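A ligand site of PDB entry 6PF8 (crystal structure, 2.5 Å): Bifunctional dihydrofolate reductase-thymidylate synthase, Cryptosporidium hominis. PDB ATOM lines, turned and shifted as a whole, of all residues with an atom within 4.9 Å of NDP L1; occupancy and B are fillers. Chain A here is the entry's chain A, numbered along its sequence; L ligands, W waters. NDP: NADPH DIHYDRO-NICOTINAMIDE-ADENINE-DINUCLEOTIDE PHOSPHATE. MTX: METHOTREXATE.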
ATOM      1  N   VAL A   9     -16.032   7.403  32.889  1.00  0.00           N
ATOM      2  CA  VAL A   9     -16.162   6.464  34.007  1.00  0.00           C
ATOM      3  C   VAL A   9     -14.771   5.938  34.312  1.00  0.00           C
ATOM      4  O   VAL A   9     -14.079   5.436  33.421  1.00  0.00           O
ATOM      5  CB  VAL A   9     -17.123   5.310  33.670  1.00  0.00           C
ATOM      6  CG1 VAL A   9     -17.451   4.513  34.924  1.00  0.00           C
ATOM      7  CG2 VAL A   9     -18.396   5.828  33.025  1.00  0.00           C
ATOM      8  N   VAL A  10     -14.365   6.041  35.578  1.00  0.00           N
ATOM      9  CA  VAL A  10     -13.015   5.668  35.977  1.00  0.00           C
ATOM     10  C   VAL A  10     -13.033   5.298  37.456  1.00  0.00           C
ATOM     11  O   VAL A  10     -13.833   5.822  38.230  1.00  0.00           O
ATOM     12  CB  VAL A  10     -12.011   6.806  35.685  1.00  0.00           C
ATOM     13  CG1 VAL A  10     -12.343   8.042  36.507  1.00  0.00           C
ATOM     14  CG2 VAL A  10     -10.573   6.355  35.931  1.00  0.00           C
ATOM     15  N   ALA A  11     -12.142   4.381  37.841  1.00  0.00           N
ATOM     16  CA  ALA A  11     -11.879   4.060  39.234  1.00  0.00           C
ATOM     17  C   ALA A  11     -10.399   4.314  39.497  1.00  0.00           C
ATOM     18  O   ALA A  11      -9.543   3.686  38.872  1.00  0.00           O
ATOM     19  CB  ALA A  11     -12.252   2.617  39.574  1.00  0.00           C
ATOM     20  N   ILE A  19      -4.714   3.819  38.296  1.00  0.00           N
ATOM     21  CA  ILE A  19      -5.860   3.086  37.746  1.00  0.00           C
ATOM     22  C   ILE A  19      -5.441   1.731  37.197  1.00  0.00           C
ATOM     23  O   ILE A  19      -6.299   0.881  36.932  1.00  0.00           O
ATOM     24  CB  ILE A  19      -6.574   3.908  36.662  1.00  0.00           C
ATOM     25  CG1 ILE A  19      -5.667   4.118  35.440  1.00  0.00           C
ATOM     26  CG2 ILE A  19      -7.046   5.254  37.205  1.00  0.00           C
ATOM     27  CD1 ILE A  19      -6.395   4.666  34.230  1.00  0.00           C
ATOM     28  N   GLY A  20      -4.149   1.500  37.008  1.00  0.00           N
ATOM     29  CA  GLY A  20      -3.713   0.266  36.385  1.00  0.00           C
ATOM     30  C   GLY A  20      -2.286  -0.099  36.708  1.00  0.00           C
ATOM     31  O   GLY A  20      -1.482   0.741  37.127  1.00  0.00           O
ATOM     32  N   ILE A  21      -1.974  -1.381  36.505  1.00  0.00           N
ATOM     33  CA  ILE A  21      -0.632  -1.896  36.718  1.00  0.00           C
ATOM     34  C   ILE A  21      -0.442  -3.174  35.899  1.00  0.00           C
ATOM     35  O   ILE A  21      -1.243  -4.110  36.006  1.00  0.00           O
ATOM     36  CB  ILE A  21      -0.361  -2.155  38.220  1.00  0.00           C
ATOM     37  CG1 ILE A  21       1.001  -2.813  38.419  1.00  0.00           C
ATOM     38  CG2 ILE A  21      -1.465  -3.009  38.830  1.00  0.00           C
ATOM     39  CD1 ILE A  21       2.164  -1.922  38.005  1.00  0.00           C
ATOM     40  N   GLY A  23      -0.973  -3.918  32.817  1.00  0.00           N
ATOM     41  CA  GLY A  23      -2.055  -4.259  31.922  1.00  0.00           C
ATOM     42  C   GLY A  23      -3.340  -4.694  32.604  1.00  0.00           C
ATOM     43  O   GLY A  23      -4.279  -5.092  31.896  1.00  0.00           O
ATOM     44  N   GLN A  24      -3.435  -4.616  33.925  1.00  0.00           N
ATOM     45  CA  GLN A  24      -4.648  -4.991  34.621  1.00  0.00           C
ATOM     46  C   GLN A  24      -4.909  -3.997  35.745  1.00  0.00           C
ATOM     47  O   GLN A  24      -4.171  -3.026  35.930  1.00  0.00           O
ATOM     48  CB  GLN A  24      -4.557  -6.428  35.141  1.00  0.00           C
ATOM     49  CG  GLN A  24      -3.500  -6.670  36.193  1.00  0.00           C
ATOM     50  CD  GLN A  24      -3.374  -8.135  36.555  1.00  0.00           C
ATOM     51  OE1 GLN A  24      -3.798  -9.015  35.796  1.00  0.00           O
ATOM     52  NE2 GLN A  24      -2.791  -8.410  37.719  1.00  0.00           N
ATOM     53  N   LEU A  25      -5.987  -4.234  36.483  1.00  0.00           N
ATOM     54  CA  LEU A  25      -6.346  -3.339  37.567  1.00  0.00           C
ATOM     55  C   LEU A  25      -5.517  -3.661  38.816  1.00  0.00           C
ATOM     56  O   LEU A  25      -5.143  -4.821  39.030  1.00  0.00           O
ATOM     57  CB  LEU A  25      -7.830  -3.457  37.893  1.00  0.00           C
ATOM     58  CG  LEU A  25      -8.814  -3.184  36.761  1.00  0.00           C
ATOM     59  CD1 LEU A  25     -10.237  -3.381  37.251  1.00  0.00           C
ATOM     60  CD2 LEU A  25      -8.613  -1.798  36.190  1.00  0.00           C
ATOM     61  N   TRP A  27      -6.620  -3.740  41.767  1.00  0.00           N
ATOM     62  CA  TRP A  27      -7.534  -4.210  42.802  1.00  0.00           C
ATOM     63  C   TRP A  27      -8.608  -5.049  42.136  1.00  0.00           C
ATOM     64  O   TRP A  27      -8.680  -5.141  40.911  1.00  0.00           O
ATOM     65  CB  TRP A  27      -8.147  -3.038  43.575  1.00  0.00           C
ATOM     66  CG  TRP A  27      -8.748  -2.001  42.678  1.00  0.00           C
ATOM     67  CD1 TRP A  27      -9.895  -2.126  41.932  1.00  0.00           C
ATOM     68  CD2 TRP A  27      -8.232  -0.696  42.404  1.00  0.00           C
ATOM     69  NE1 TRP A  27     -10.114  -0.967  41.226  1.00  0.00           N
ATOM     70  CE2 TRP A  27      -9.108  -0.078  41.494  1.00  0.00           C
ATOM     71  CE3 TRP A  27      -7.108   0.008  42.854  1.00  0.00           C
ATOM     72  CZ2 TRP A  27      -8.900   1.216  41.024  1.00  0.00           C
ATOM     73  CZ3 TRP A  27      -6.911   1.295  42.379  1.00  0.00           C
ATOM     74  CH2 TRP A  27      -7.801   1.888  41.476  1.00  0.00           C
ATOM     75  N   GLY A  55      -9.380   2.594  24.862  1.00  0.00           N
ATOM     76  CA  GLY A  55      -8.150   2.360  24.141  1.00  0.00           C
ATOM     77  C   GLY A  55      -7.922   0.885  23.845  1.00  0.00           C
ATOM     78  O   GLY A  55      -8.587   0.000  24.376  1.00  0.00           O
ATOM     79  N   ARG A  56      -6.932   0.633  22.988  1.00  0.00           N
ATOM     80  CA  ARG A  56      -6.696  -0.738  22.536  1.00  0.00           C
ATOM     81  C   ARG A  56      -6.147  -1.614  23.657  1.00  0.00           C
ATOM     82  O   ARG A  56      -6.486  -2.795  23.752  1.00  0.00           O
ATOM     83  CB  ARG A  56      -5.722  -0.750  21.349  1.00  0.00           C
ATOM     84  CG  ARG A  56      -5.613  -2.105  20.681  1.00  0.00           C
ATOM     85  CD  ARG A  56      -4.178  -2.432  20.338  1.00  0.00           C
ATOM     86  NE  ARG A  56      -3.414  -2.850  21.499  1.00  0.00           N
ATOM     87  CZ  ARG A  56      -2.118  -2.644  21.663  1.00  0.00           C
ATOM     88  NH1 ARG A  56      -1.429  -1.991  20.729  1.00  0.00           N
ATOM     89  NH2 ARG A  56      -1.504  -3.060  22.760  1.00  0.00           N
ATOM     90  N   LYS A  57      -5.294  -1.056  24.521  1.00  0.00           N
ATOM     91  CA  LYS A  57      -4.758  -1.850  25.619  1.00  0.00           C
ATOM     92  C   LYS A  57      -5.836  -2.223  26.613  1.00  0.00           C
ATOM     93  O   LYS A  57      -5.826  -3.327  27.169  1.00  0.00           O
ATOM     94  CB  LYS A  57      -3.612  -1.102  26.304  1.00  0.00           C
ATOM     95  CG  LYS A  57      -2.396  -0.891  25.403  1.00  0.00           C
ATOM     96  CD  LYS A  57      -1.224  -0.305  26.181  1.00  0.00           C
ATOM     97  CE  LYS A  57      -0.028  -0.072  25.278  1.00  0.00           C
ATOM     98  NZ  LYS A  57       1.112   0.499  26.026  1.00  0.00           N
ATOM     99  N   THR A  58      -6.797  -1.326  26.846  1.00  0.00           N
ATOM    100  CA  THR A  58      -7.950  -1.676  27.661  1.00  0.00           C
ATOM    101  C   THR A  58      -8.823  -2.713  26.960  1.00  0.00           C
ATOM    102  O   THR A  58      -9.370  -3.613  27.613  1.00  0.00           O
ATOM    103  CB  THR A  58      -8.752  -0.414  27.998  1.00  0.00           C
ATOM    104  OG1 THR A  58      -7.924   0.491  28.727  1.00  0.00           O
ATOM    105  CG2 THR A  58      -9.974  -0.758  28.827  1.00  0.00           C
ATOM    106  N   SER A  61      -7.271  -5.901  27.742  1.00  0.00           N
ATOM    107  CA  SER A  61      -7.396  -6.323  29.128  1.00  0.00           C
ATOM    108  C   SER A  61      -8.758  -6.925  29.455  1.00  0.00           C
ATOM    109  O   SER A  61      -8.879  -7.680  30.421  1.00  0.00           O
ATOM    110  CB  SER A  61      -7.122  -5.148  30.071  1.00  0.00           C
ATOM    111  OG  SER A  61      -8.134  -4.169  29.970  1.00  0.00           O
ATOM    112  N   ILE A  75     -10.215   2.625  20.105  1.00  0.00           N
ATOM    113  CA  ILE A  75      -9.313   3.563  19.462  1.00  0.00           C
ATOM    114  C   ILE A  75      -7.979   2.847  19.240  1.00  0.00           C
ATOM    115  O   ILE A  75      -7.336   2.408  20.187  1.00  0.00           O
ATOM    116  CB  ILE A  75      -9.122   4.823  20.307  1.00  0.00           C
ATOM    117  CG1 ILE A  75     -10.486   5.439  20.649  1.00  0.00           C
ATOM    118  CG2 ILE A  75      -8.247   5.833  19.577  1.00  0.00           C
ATOM    119  CD1 ILE A  75     -11.332   5.760  19.447  1.00  0.00           C
ATOM    120  N   SER A  76      -7.579   2.729  17.974  1.00  0.00           N
ATOM    121  CA  SER A  76      -6.347   2.014  17.655  1.00  0.00           C
ATOM    122  C   SER A  76      -5.862   2.437  16.278  1.00  0.00           C
ATOM    123  O   SER A  76      -6.664   2.756  15.392  1.00  0.00           O
ATOM    124  CB  SER A  76      -6.553   0.490  17.689  1.00  0.00           C
ATOM    125  OG  SER A  76      -5.374  -0.190  17.272  1.00  0.00           O
ATOM    126  N   SER A  77      -4.542   2.442  16.106  1.00  0.00           N
ATOM    127  CA  SER A  77      -3.948   2.740  14.819  1.00  0.00           C
ATOM    128  C   SER A  77      -3.697   1.501  13.963  1.00  0.00           C
ATOM    129  O   SER A  77      -3.571   1.622  12.746  1.00  0.00           O
ATOM    130  CB  SER A  77      -2.619   3.484  15.010  1.00  0.00           C
ATOM    131  OG  SER A  77      -1.680   2.691  15.711  1.00  0.00           O
ATOM    132  N   SER A  78      -3.645   0.312  14.584  1.00  0.00           N
ATOM    133  CA  SER A  78      -3.295  -0.905  13.865  1.00  0.00           C
ATOM    134  C   SER A  78      -4.417  -1.923  13.786  1.00  0.00           C
ATOM    135  O   SER A  78      -4.379  -2.790  12.906  1.00  0.00           O
ATOM    136  CB  SER A  78      -2.077  -1.575  14.529  1.00  0.00           C
ATOM    137  OG  SER A  78      -2.358  -1.915  15.878  1.00  0.00           O
ATOM    138  N   LEU A  79      -5.413  -1.849  14.662  1.00  0.00           N
ATOM    139  CA  LEU A  79      -6.481  -2.838  14.664  1.00  0.00           C
ATOM    140  C   LEU A  79      -7.248  -2.778  13.344  1.00  0.00           C
ATOM    141  O   LEU A  79      -7.520  -1.686  12.835  1.00  0.00           O
ATOM    142  CB  LEU A  79      -7.437  -2.608  15.829  1.00  0.00           C
ATOM    143  CG  LEU A  79      -7.163  -3.383  17.127  1.00  0.00           C
ATOM    144  CD1 LEU A  79      -8.268  -3.120  18.133  1.00  0.00           C
ATOM    145  CD2 LEU A  79      -7.030  -4.871  16.852  1.00  0.00           C
ATOM    146  N   ARG A  92      -9.535   5.416  14.215  1.00  0.00           N
ATOM    147  CA  ARG A  92      -8.096   5.696  14.208  1.00  0.00           C
ATOM    148  C   ARG A  92      -7.693   6.798  15.174  1.00  0.00           C
ATOM    149  O   ARG A  92      -6.499   6.918  15.464  1.00  0.00           O
ATOM    150  CB  ARG A  92      -7.641   6.077  12.793  1.00  0.00           C
ATOM    151  CG  ARG A  92      -7.769   4.967  11.776  1.00  0.00           C
ATOM    152  CD  ARG A  92      -7.040   3.712  12.226  1.00  0.00           C
ATOM    153  NE  ARG A  92      -7.290   2.568  11.354  1.00  0.00           N
ATOM    154  CZ  ARG A  92      -7.047   1.311  11.678  1.00  0.00           C
ATOM    155  NH1 ARG A  92      -6.540   1.013  12.870  1.00  0.00           N
ATOM    156  NH2 ARG A  92      -7.315   0.332  10.822  1.00  0.00           N
ATOM    157  N   ASN A  93      -8.625   7.600  15.659  1.00  0.00           N
ATOM    158  CA  ASN A  93      -8.316   8.629  16.645  1.00  0.00           C
ATOM    159  C   ASN A  93      -9.576   8.944  17.431  1.00  0.00           C
ATOM    160  O   ASN A  93     -10.696   8.599  17.023  1.00  0.00           O
ATOM    161  CB  ASN A  93      -7.723   9.878  15.988  1.00  0.00           C
ATOM    162  CG  ASN A  93      -8.677  10.515  15.003  1.00  0.00           C
ATOM    163  OD1 ASN A  93      -9.521  11.332  15.372  1.00  0.00           O
ATOM    164  ND2 ASN A  93      -8.543  10.163  13.732  1.00  0.00           N
ATOM    165  N   CYS A 113     -14.309   5.156  28.565  1.00  0.00           N
ATOM    166  CA  CYS A 113     -14.320   4.062  29.522  1.00  0.00           C
ATOM    167  C   CYS A 113     -12.950   3.620  30.000  1.00  0.00           C
ATOM    168  O   CYS A 113     -12.876   2.733  30.864  1.00  0.00           O
ATOM    169  CB  CYS A 113     -15.046   2.852  28.931  1.00  0.00           C
ATOM    170  SG  CYS A 113     -16.825   3.050  28.926  1.00  0.00           S
ATOM    171  N   GLY A 114     -11.866   4.177  29.496  1.00  0.00           N
ATOM    172  CA  GLY A 114     -10.600   3.797  30.081  1.00  0.00           C
ATOM    173  C   GLY A 114      -9.419   3.925  29.153  1.00  0.00           C
ATOM    174  O   GLY A 114      -9.544   3.978  27.929  1.00  0.00           O
ATOM    175  N   GLY A 115      -8.245   3.903  29.762  1.00  0.00           N
ATOM    176  CA  GLY A 115      -6.995   4.210  29.098  1.00  0.00           C
ATOM    177  C   GLY A 115      -6.537   5.595  29.483  1.00  0.00           C
ATOM    178  O   GLY A 115      -7.236   6.574  29.223  1.00  0.00           O
ATOM    179  N   GLU A 116      -5.374   5.688  30.148  1.00  0.00           N
ATOM    180  CA  GLU A 116      -4.821   6.994  30.474  1.00  0.00           C
ATOM    181  C   GLU A 116      -4.651   7.839  29.220  1.00  0.00           C
ATOM    182  O   GLU A 116      -4.911   9.052  29.237  1.00  0.00           O
ATOM    183  CB  GLU A 116      -3.485   6.840  31.204  1.00  0.00           C
ATOM    184  CG  GLU A 116      -2.709   8.144  31.361  1.00  0.00           C
ATOM    185  CD  GLU A 116      -1.518   8.005  32.286  1.00  0.00           C
ATOM    186  OE1 GLU A 116      -1.329   6.907  32.864  1.00  0.00           O
ATOM    187  OE2 GLU A 116      -0.764   8.991  32.429  1.00  0.00           O
ATOM    188  N   SER A 117      -4.241   7.224  28.110  1.00  0.00           N
ATOM    189  CA  SER A 117      -4.099   7.968  26.860  1.00  0.00           C
ATOM    190  C   SER A 117      -5.461   8.473  26.374  1.00  0.00           C
ATOM    191  O   SER A 117      -5.560   9.605  25.872  1.00  0.00           O
ATOM    192  CB  SER A 117      -3.445   7.088  25.796  1.00  0.00           C
ATOM    193  OG  SER A 117      -4.237   5.965  25.470  1.00  0.00           O
ATOM    194  N   ILE A 118      -6.501   7.660  26.508  1.00  0.00           N
ATOM    195  CA  ILE A 118      -7.828   8.078  26.067  1.00  0.00           C
ATOM    196  C   ILE A 118      -8.413   9.121  27.012  1.00  0.00           C
ATOM    197  O   ILE A 118      -9.013  10.105  26.580  1.00  0.00           O
ATOM    198  CB  ILE A 118      -8.753   6.856  25.924  1.00  0.00           C
ATOM    199  CG1 ILE A 118      -8.098   5.811  25.022  1.00  0.00           C
ATOM    200  CG2 ILE A 118     -10.099   7.267  25.341  1.00  0.00           C
ATOM    201  CD1 ILE A 118      -7.805   6.295  23.624  1.00  0.00           C
ATOM    202  N   TYR A 119      -8.257   8.915  28.326  1.00  0.00           N
ATOM    203  CA  TYR A 119      -8.723   9.895  29.308  1.00  0.00           C
ATOM    204  C   TYR A 119      -8.054  11.249  29.078  1.00  0.00           C
ATOM    205  O   TYR A 119      -8.721  12.293  29.063  1.00  0.00           O
ATOM    206  CB  TYR A 119      -8.438   9.418  30.727  1.00  0.00           C
ATOM    207  CG  TYR A 119      -9.320   8.318  31.251  1.00  0.00           C
ATOM    208  CD1 TYR A 119     -10.676   8.269  30.956  1.00  0.00           C
ATOM    209  CD2 TYR A 119      -8.799   7.324  32.068  1.00  0.00           C
ATOM    210  CE1 TYR A 119     -11.479   7.259  31.451  1.00  0.00           C
ATOM    211  CE2 TYR A 119      -9.589   6.307  32.563  1.00  0.00           C
ATOM    212  CZ  TYR A 119     -10.932   6.284  32.260  1.00  0.00           C
ATOM    213  OH  TYR A 119     -11.709   5.261  32.756  1.00  0.00           O
ATOM    214  N   ASP A 121      -6.582  12.555  26.449  1.00  0.00           N
ATOM    215  CA  ASP A 121      -6.971  13.233  25.215  1.00  0.00           C
ATOM    216  C   ASP A 121      -8.419  13.714  25.262  1.00  0.00           C
ATOM    217  O   ASP A 121      -8.744  14.750  24.663  1.00  0.00           O
ATOM    218  CB  ASP A 121      -6.760  12.312  24.015  1.00  0.00           C
ATOM    219  CG  ASP A 121      -5.295  12.163  23.657  1.00  0.00           C
ATOM    220  OD1 ASP A 121      -4.495  13.071  23.980  1.00  0.00           O
ATOM    221  OD2 ASP A 121      -4.923  11.129  23.047  1.00  0.00           O
ATOM    222  N   THR A 145      -0.252   3.335  35.501  1.00  0.00           N
ATOM    223  CA  THR A 145      -1.250   4.043  34.724  1.00  0.00           C
ATOM    224  C   THR A 145      -2.054   4.925  35.680  1.00  0.00           C
ATOM    225  O   THR A 145      -2.393   4.488  36.787  1.00  0.00           O
ATOM    226  CB  THR A 145      -2.173   3.078  33.975  1.00  0.00           C
ATOM    227  OG1 THR A 145      -1.372   2.100  33.290  1.00  0.00           O
ATOM    228  CG2 THR A 145      -3.013   3.809  32.956  1.00  0.00           C
HETATM  229  PA  NDP L   1      -4.960   2.491  26.618  1.00  0.00           P
HETATM  230  O1A NDP L   1      -5.144   3.985  26.657  1.00  0.00           O
HETATM  231  O2A NDP L   1      -6.176   1.802  27.152  1.00  0.00           O
HETATM  232  O5B NDP L   1      -4.774   2.036  25.168  1.00  0.00           O
HETATM  233  C5B NDP L   1      -3.774   2.613  24.377  1.00  0.00           C
HETATM  234  C4B NDP L   1      -3.857   2.347  22.929  1.00  0.00           C
HETATM  235  O4B NDP L   1      -4.932   3.076  22.367  1.00  0.00           O
HETATM  236  C3B NDP L   1      -2.682   2.800  22.190  1.00  0.00           C
HETATM  237  O3B NDP L   1      -1.637   1.884  22.244  1.00  0.00           O
HETATM  238  C2B NDP L   1      -3.206   2.913  20.852  1.00  0.00           C
HETATM  239  O2B NDP L   1      -3.400   1.649  20.271  1.00  0.00           O
HETATM  240  C1B NDP L   1      -4.518   3.503  21.078  1.00  0.00           C
HETATM  241  N9A NDP L   1      -4.428   4.911  21.033  1.00  0.00           N
HETATM  242  C8A NDP L   1      -4.333   5.746  22.087  1.00  0.00           C
HETATM  243  N7A NDP L   1      -4.271   7.019  21.645  1.00  0.00           N
HETATM  244  C5A NDP L   1      -4.326   7.006  20.276  1.00  0.00           C
HETATM  245  C6A NDP L   1      -4.304   7.998  19.267  1.00  0.00           C
HETATM  246  N6A NDP L   1      -4.197   9.429  19.660  1.00  0.00           N
HETATM  247  N1A NDP L   1      -4.387   7.643  17.957  1.00  0.00           N
HETATM  248  C2A NDP L   1      -4.482   6.328  17.624  1.00  0.00           C
HETATM  249  N3A NDP L   1      -4.512   5.349  18.543  1.00  0.00           N
HETATM  250  C4A NDP L   1      -4.427   5.665  19.884  1.00  0.00           C
HETATM  251  O3  NDP L   1      -3.672   2.031  27.452  1.00  0.00           O
HETATM  252  PN  NDP L   1      -3.346   2.535  28.913  1.00  0.00           P
HETATM  253  O1N NDP L   1      -1.970   2.012  29.365  1.00  0.00           O
HETATM  254  O2N NDP L   1      -3.286   4.053  28.955  1.00  0.00           O
HETATM  255  O5D NDP L   1      -4.504   1.993  29.904  1.00  0.00           O
HETATM  256  C5D NDP L   1      -4.542   0.643  30.287  1.00  0.00           C
HETATM  257  C4D NDP L   1      -4.339   0.361  31.707  1.00  0.00           C
HETATM  258  O4D NDP L   1      -5.246   1.152  32.484  1.00  0.00           O
HETATM  259  C3D NDP L   1      -4.646  -1.048  32.004  1.00  0.00           C
HETATM  260  O3D NDP L   1      -3.875  -1.469  33.084  1.00  0.00           O
HETATM  261  C2D NDP L   1      -6.025  -1.010  32.377  1.00  0.00           C
HETATM  262  O2D NDP L   1      -6.352  -2.099  33.179  1.00  0.00           O
HETATM  263  C1D NDP L   1      -6.113   0.263  33.119  1.00  0.00           C
HETATM  264  N1N NDP L   1      -7.457   0.746  33.118  1.00  0.00           N
HETATM  265  C2N NDP L   1      -8.000   1.155  34.283  1.00  0.00           C
HETATM  266  C3N NDP L   1      -9.307   1.645  34.334  1.00  0.00           C
HETATM  267  C7N NDP L   1      -9.890   2.087  35.663  1.00  0.00           C
HETATM  268  O7N NDP L   1     -10.976   2.696  35.677  1.00  0.00           O
HETATM  269  N7N NDP L   1      -9.217   1.832  36.900  1.00  0.00           N
HETATM  270  C4N NDP L   1     -10.067   1.705  33.151  1.00  0.00           C
HETATM  271  C5N NDP L   1      -9.478   1.278  31.964  1.00  0.00           C
HETATM  272  C6N NDP L   1      -8.166   0.796  31.954  1.00  0.00           C
HETATM  273  P2B NDP L   1      -2.470   1.097  19.153  1.00  0.00           P
HETATM  274  O1X NDP L   1      -1.097   0.739  19.765  1.00  0.00           O
HETATM  275  O2X NDP L   1      -3.079  -0.104  18.561  1.00  0.00           O
HETATM  276  O3X NDP L   1      -2.290   2.116  18.077  1.00  0.00           O
HETATM  277  N1  MTX L   2     -14.291   0.845  37.136  1.00  0.00           N
HETATM  278  C2  MTX L   2     -14.847   2.068  37.053  1.00  0.00           C
HETATM  279  NA2 MTX L   2     -15.479   2.627  38.215  1.00  0.00           N
HETATM  280  N3  MTX L   2     -14.851   2.781  35.914  1.00  0.00           N
HETATM  281  C4  MTX L   2     -14.274   2.285  34.794  1.00  0.00           C
HETATM  282  NA4 MTX L   2     -14.250   3.005  33.570  1.00  0.00           N
HETATM  283  C4A MTX L   2     -13.669   1.016  34.846  1.00  0.00           C
HETATM  284  N5  MTX L   2     -13.088   0.497  33.731  1.00  0.00           N
HETATM  285  C6  MTX L   2     -12.517  -0.714  33.803  1.00  0.00           C
HETATM  286  C7  MTX L   2     -12.514  -1.458  34.993  1.00  0.00           C
HETATM  287  N8  MTX L   2     -13.116  -0.934  36.087  1.00  0.00           N
HETATM  288  C8A MTX L   2     -13.695   0.309  36.031  1.00  0.00           C
HETATM  289  C9  MTX L   2     -11.879  -1.277  32.560  1.00  0.00           C
HETATM  290  N10 MTX L   2     -11.912  -2.714  32.525  1.00  0.00           N
HETATM  291  CM  MTX L   2     -10.667  -3.446  32.536  1.00  0.00           C
HETATM  292  C11 MTX L   2     -15.594  -4.811  32.615  1.00  0.00           C
HETATM  293  C12 MTX L   2     -14.475  -5.288  33.283  1.00  0.00           C
HETATM  294  C13 MTX L   2     -13.274  -4.594  33.230  1.00  0.00           C
HETATM  295  C14 MTX L   2     -13.191  -3.405  32.528  1.00  0.00           C
HETATM  296  C15 MTX L   2     -14.319  -2.899  31.862  1.00  0.00           C
HETATM  297  C16 MTX L   2     -15.519  -3.607  31.910  1.00  0.00           C
HETATM  298  C   MTX L   2     -16.865  -5.607  32.713  1.00  0.00           C
HETATM  299  O   MTX L   2     -16.793  -6.810  32.876  1.00  0.00           O
HETATM  300  N   MTX L   2     -18.176  -5.003  32.666  1.00  0.00           N
HETATM  301  CA  MTX L   2     -19.339  -5.837  32.790  1.00  0.00           C
HETATM  302  CT  MTX L   2     -20.492  -5.117  32.217  1.00  0.00           C
HETATM  303  O1  MTX L   2     -20.375  -3.890  31.954  1.00  0.00           O
HETATM  304  O2  MTX L   2     -21.574  -5.724  31.981  1.00  0.00           O
HETATM  305  CB  MTX L   2     -19.590  -5.996  34.255  1.00  0.00           C
HETATM  306  CG  MTX L   2     -19.944  -7.322  34.837  1.00  0.00           C
HETATM  307  CD  MTX L   2     -20.399  -7.291  36.267  1.00  0.00           C
HETATM  308  OE1 MTX L   2     -21.615  -7.128  36.521  1.00  0.00           O
HETATM  309  OE2 MTX L   2     -19.620  -7.684  37.173  1.00  0.00           O
HETATM  310  O   HOH W   1      -4.004   6.335  14.293  1.00  0.00           O
HETATM  311  O   HOH W   2      -0.377   3.000  30.930  1.00  0.00           O
HETATM  312  O   HOH W   3      -0.882   5.466  29.304  1.00  0.00           O
HETATM  313  O   HOH W   4      -1.006  -1.082  32.774  1.00  0.00           O
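Water W2 bridges an oxygen (O1N) of NDP L1 (2.4 Å) and the side-chain hydroxyl of Thr 145 (2.7 Å).
Water W4 lies within hydrogen-bond range of N of Gly 23 (2.8 Å), O3D of NDP L1 (2.9 Å) and OG1 of Thr 145 (3.2 Å).
N of Ser 117 lies within hydrogen-bond range of O2N of NDP L1 (3.4 Å).
The side-chain hydroxyl of Ser 117 is in hydrogen-bond range of an oxygen (O1A) of NDP L1, at 2.5 Å.
O3X of NDP L1 lies within hydrogen-bond range of N of Ser 77.
OG of Ser 77 is in hydrogen-bond range of O3X of NDP L1, at 2.5 Å.
An oxygen (O2X) of NDP L1 is in hydrogen-bond range of the side-chain hydroxyl (OG) of Ser 76, 2.6 Å away.
The backbone NH (N) of Thr 58 is in hydrogen-bond range of an oxygen (O2A) of NDP L1, 3.2 Å away.
The side-chain hydroxyl (OG1) of Thr 58 is in hydrogen-bond range of an oxygen (O2A) of NDP L1 (2.7 Å).
N of Ala 11 is in hydrogen-bond range of O7N of NDP L1 (3.0 Å).
The backbone carbonyl oxygen of Ala 11 lies within hydrogen-bond range of a nitrogen (N7N) of NDP L1, 2.7 Å away.
O2N of NDP L1 lies within hydrogen-bond range of N of Glu 116.
N of Arg 56 is in hydrogen-bond range of O4B of NDP L1 (3.2 Å).
The guanidinium group (NH1) of Arg 56 lies within salt-bridge range of an oxygen (O1X) of NDP L1, at 2.9 Å.
A nitrogen (N7N) of NDP L1 lies within hydrogen-bond range of the backbone carbonyl oxygen of Ile 19 (3.1 Å).
The backbone NH (N) of Lys 57 is in hydrogen-bond range of an oxygen (O5B) of NDP L1 (3.2 Å).
N of Gln 24 lies within hydrogen-bond range of O3D of NDP L1, 3.3 Å away.
The backbone carbonyl oxygen (O) of Gln 24 is in hydrogen-bond range of an oxygen (O3D) of NDP L1 (3.3 Å).
O2X of NDP L1 sits at hydrogen-bond distance from OG of Ser 78 (3.3 Å).
The backbone NH (N) of Val 10 sits at hydrogen-bond distance from a nitrogen (N3) of MTX L2.
A nitrogen (NA4) of MTX L2 lies within hydrogen-bond range of the backbone carbonyl oxygen of Cys 113 (3.0 Å).
The side-chain hydroxyl (OH) of Tyr 119 sits at hydrogen-bond distance from a nitrogen (NA4) of MTX L2, at 3.5 Å.
O of Val 9 lies within hydrogen-bond range of NA4 of MTX L2 (2.4 Å).
An oxygen (O4B) of NDP L1 lies close to the backbone carbonyl oxygen (O) of Ile 75, at 3.3 Å.
The backbone carbonyl oxygen (O) of Arg 92 sits close to a nitrogen (N1A) of NDP L1.
Residues that only touch NDP L1: Val 10 (3.6 Å), Gly 20 (3.7 Å), Ile 21 (3.9 Å), Gly 23 (3.3 Å), Leu 25 (3.6 Å), Gly 55 (3.5 Å), Cys 113 (3.8 Å), Gly 114 (3.3 Å), Gly 115 (3.1 Å), Ile 118 (3.8 Å), Tyr 119 (3.9 Å), Asp 121 (3.9 Å) and Thr 145 (3.5 Å).
Hydrophobic or aromatic side chains that line NDP L1: Val 10, Ile 19, Leu 25, Ile 75 and Ile 118.
26 residues have an atom within 4 Å of NDP L1: Val 10, Ala 11, Ile 19, Gly 20, Ile 21, Gly 23, Gln 24, Leu 25, Gly 55, Arg 56, Lys 57, Thr 58, Ile 75, Ser 76, Ser 77, Ser 78, Arg 92, Cys 113, Gly 114, Gly 115, Glu 116, Ser 117, Ile 118, Tyr 119, Asp 121 and Thr 145.
O of Ser 76 is in hydrogen-bond range of NH1 of Arg 92, 3.1 Å away.
The backbone NH (N) of Ser 78 lies within hydrogen-bond range of the side-chain hydroxyl (OG) of Ser 76.
N of Leu 79 lies within hydrogen-bond range of OG of Ser 76.
The backbone carbonyl oxygen of Thr 58 lies within hydrogen-bond range of the side-chain hydroxyl of Ser 61, 2.7 Å away.
The backbone NH of Arg 56 lies within hydrogen-bond range of the backbone carbonyl oxygen of Ile 75 (3.3 Å).
N of Gly 55 lies within hydrogen-bond range of O of Gly 114, at 3.4 Å.
The backbone NH (N) of Gly 114 lies close to the side-chain hydroxyl (OH) of Tyr 119.
The backbone carbonyl oxygen (O) of Val 9 sits at hydrogen-bond distance from the side-chain hydroxyl (OH) of Tyr 119, at 2.5 Å.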
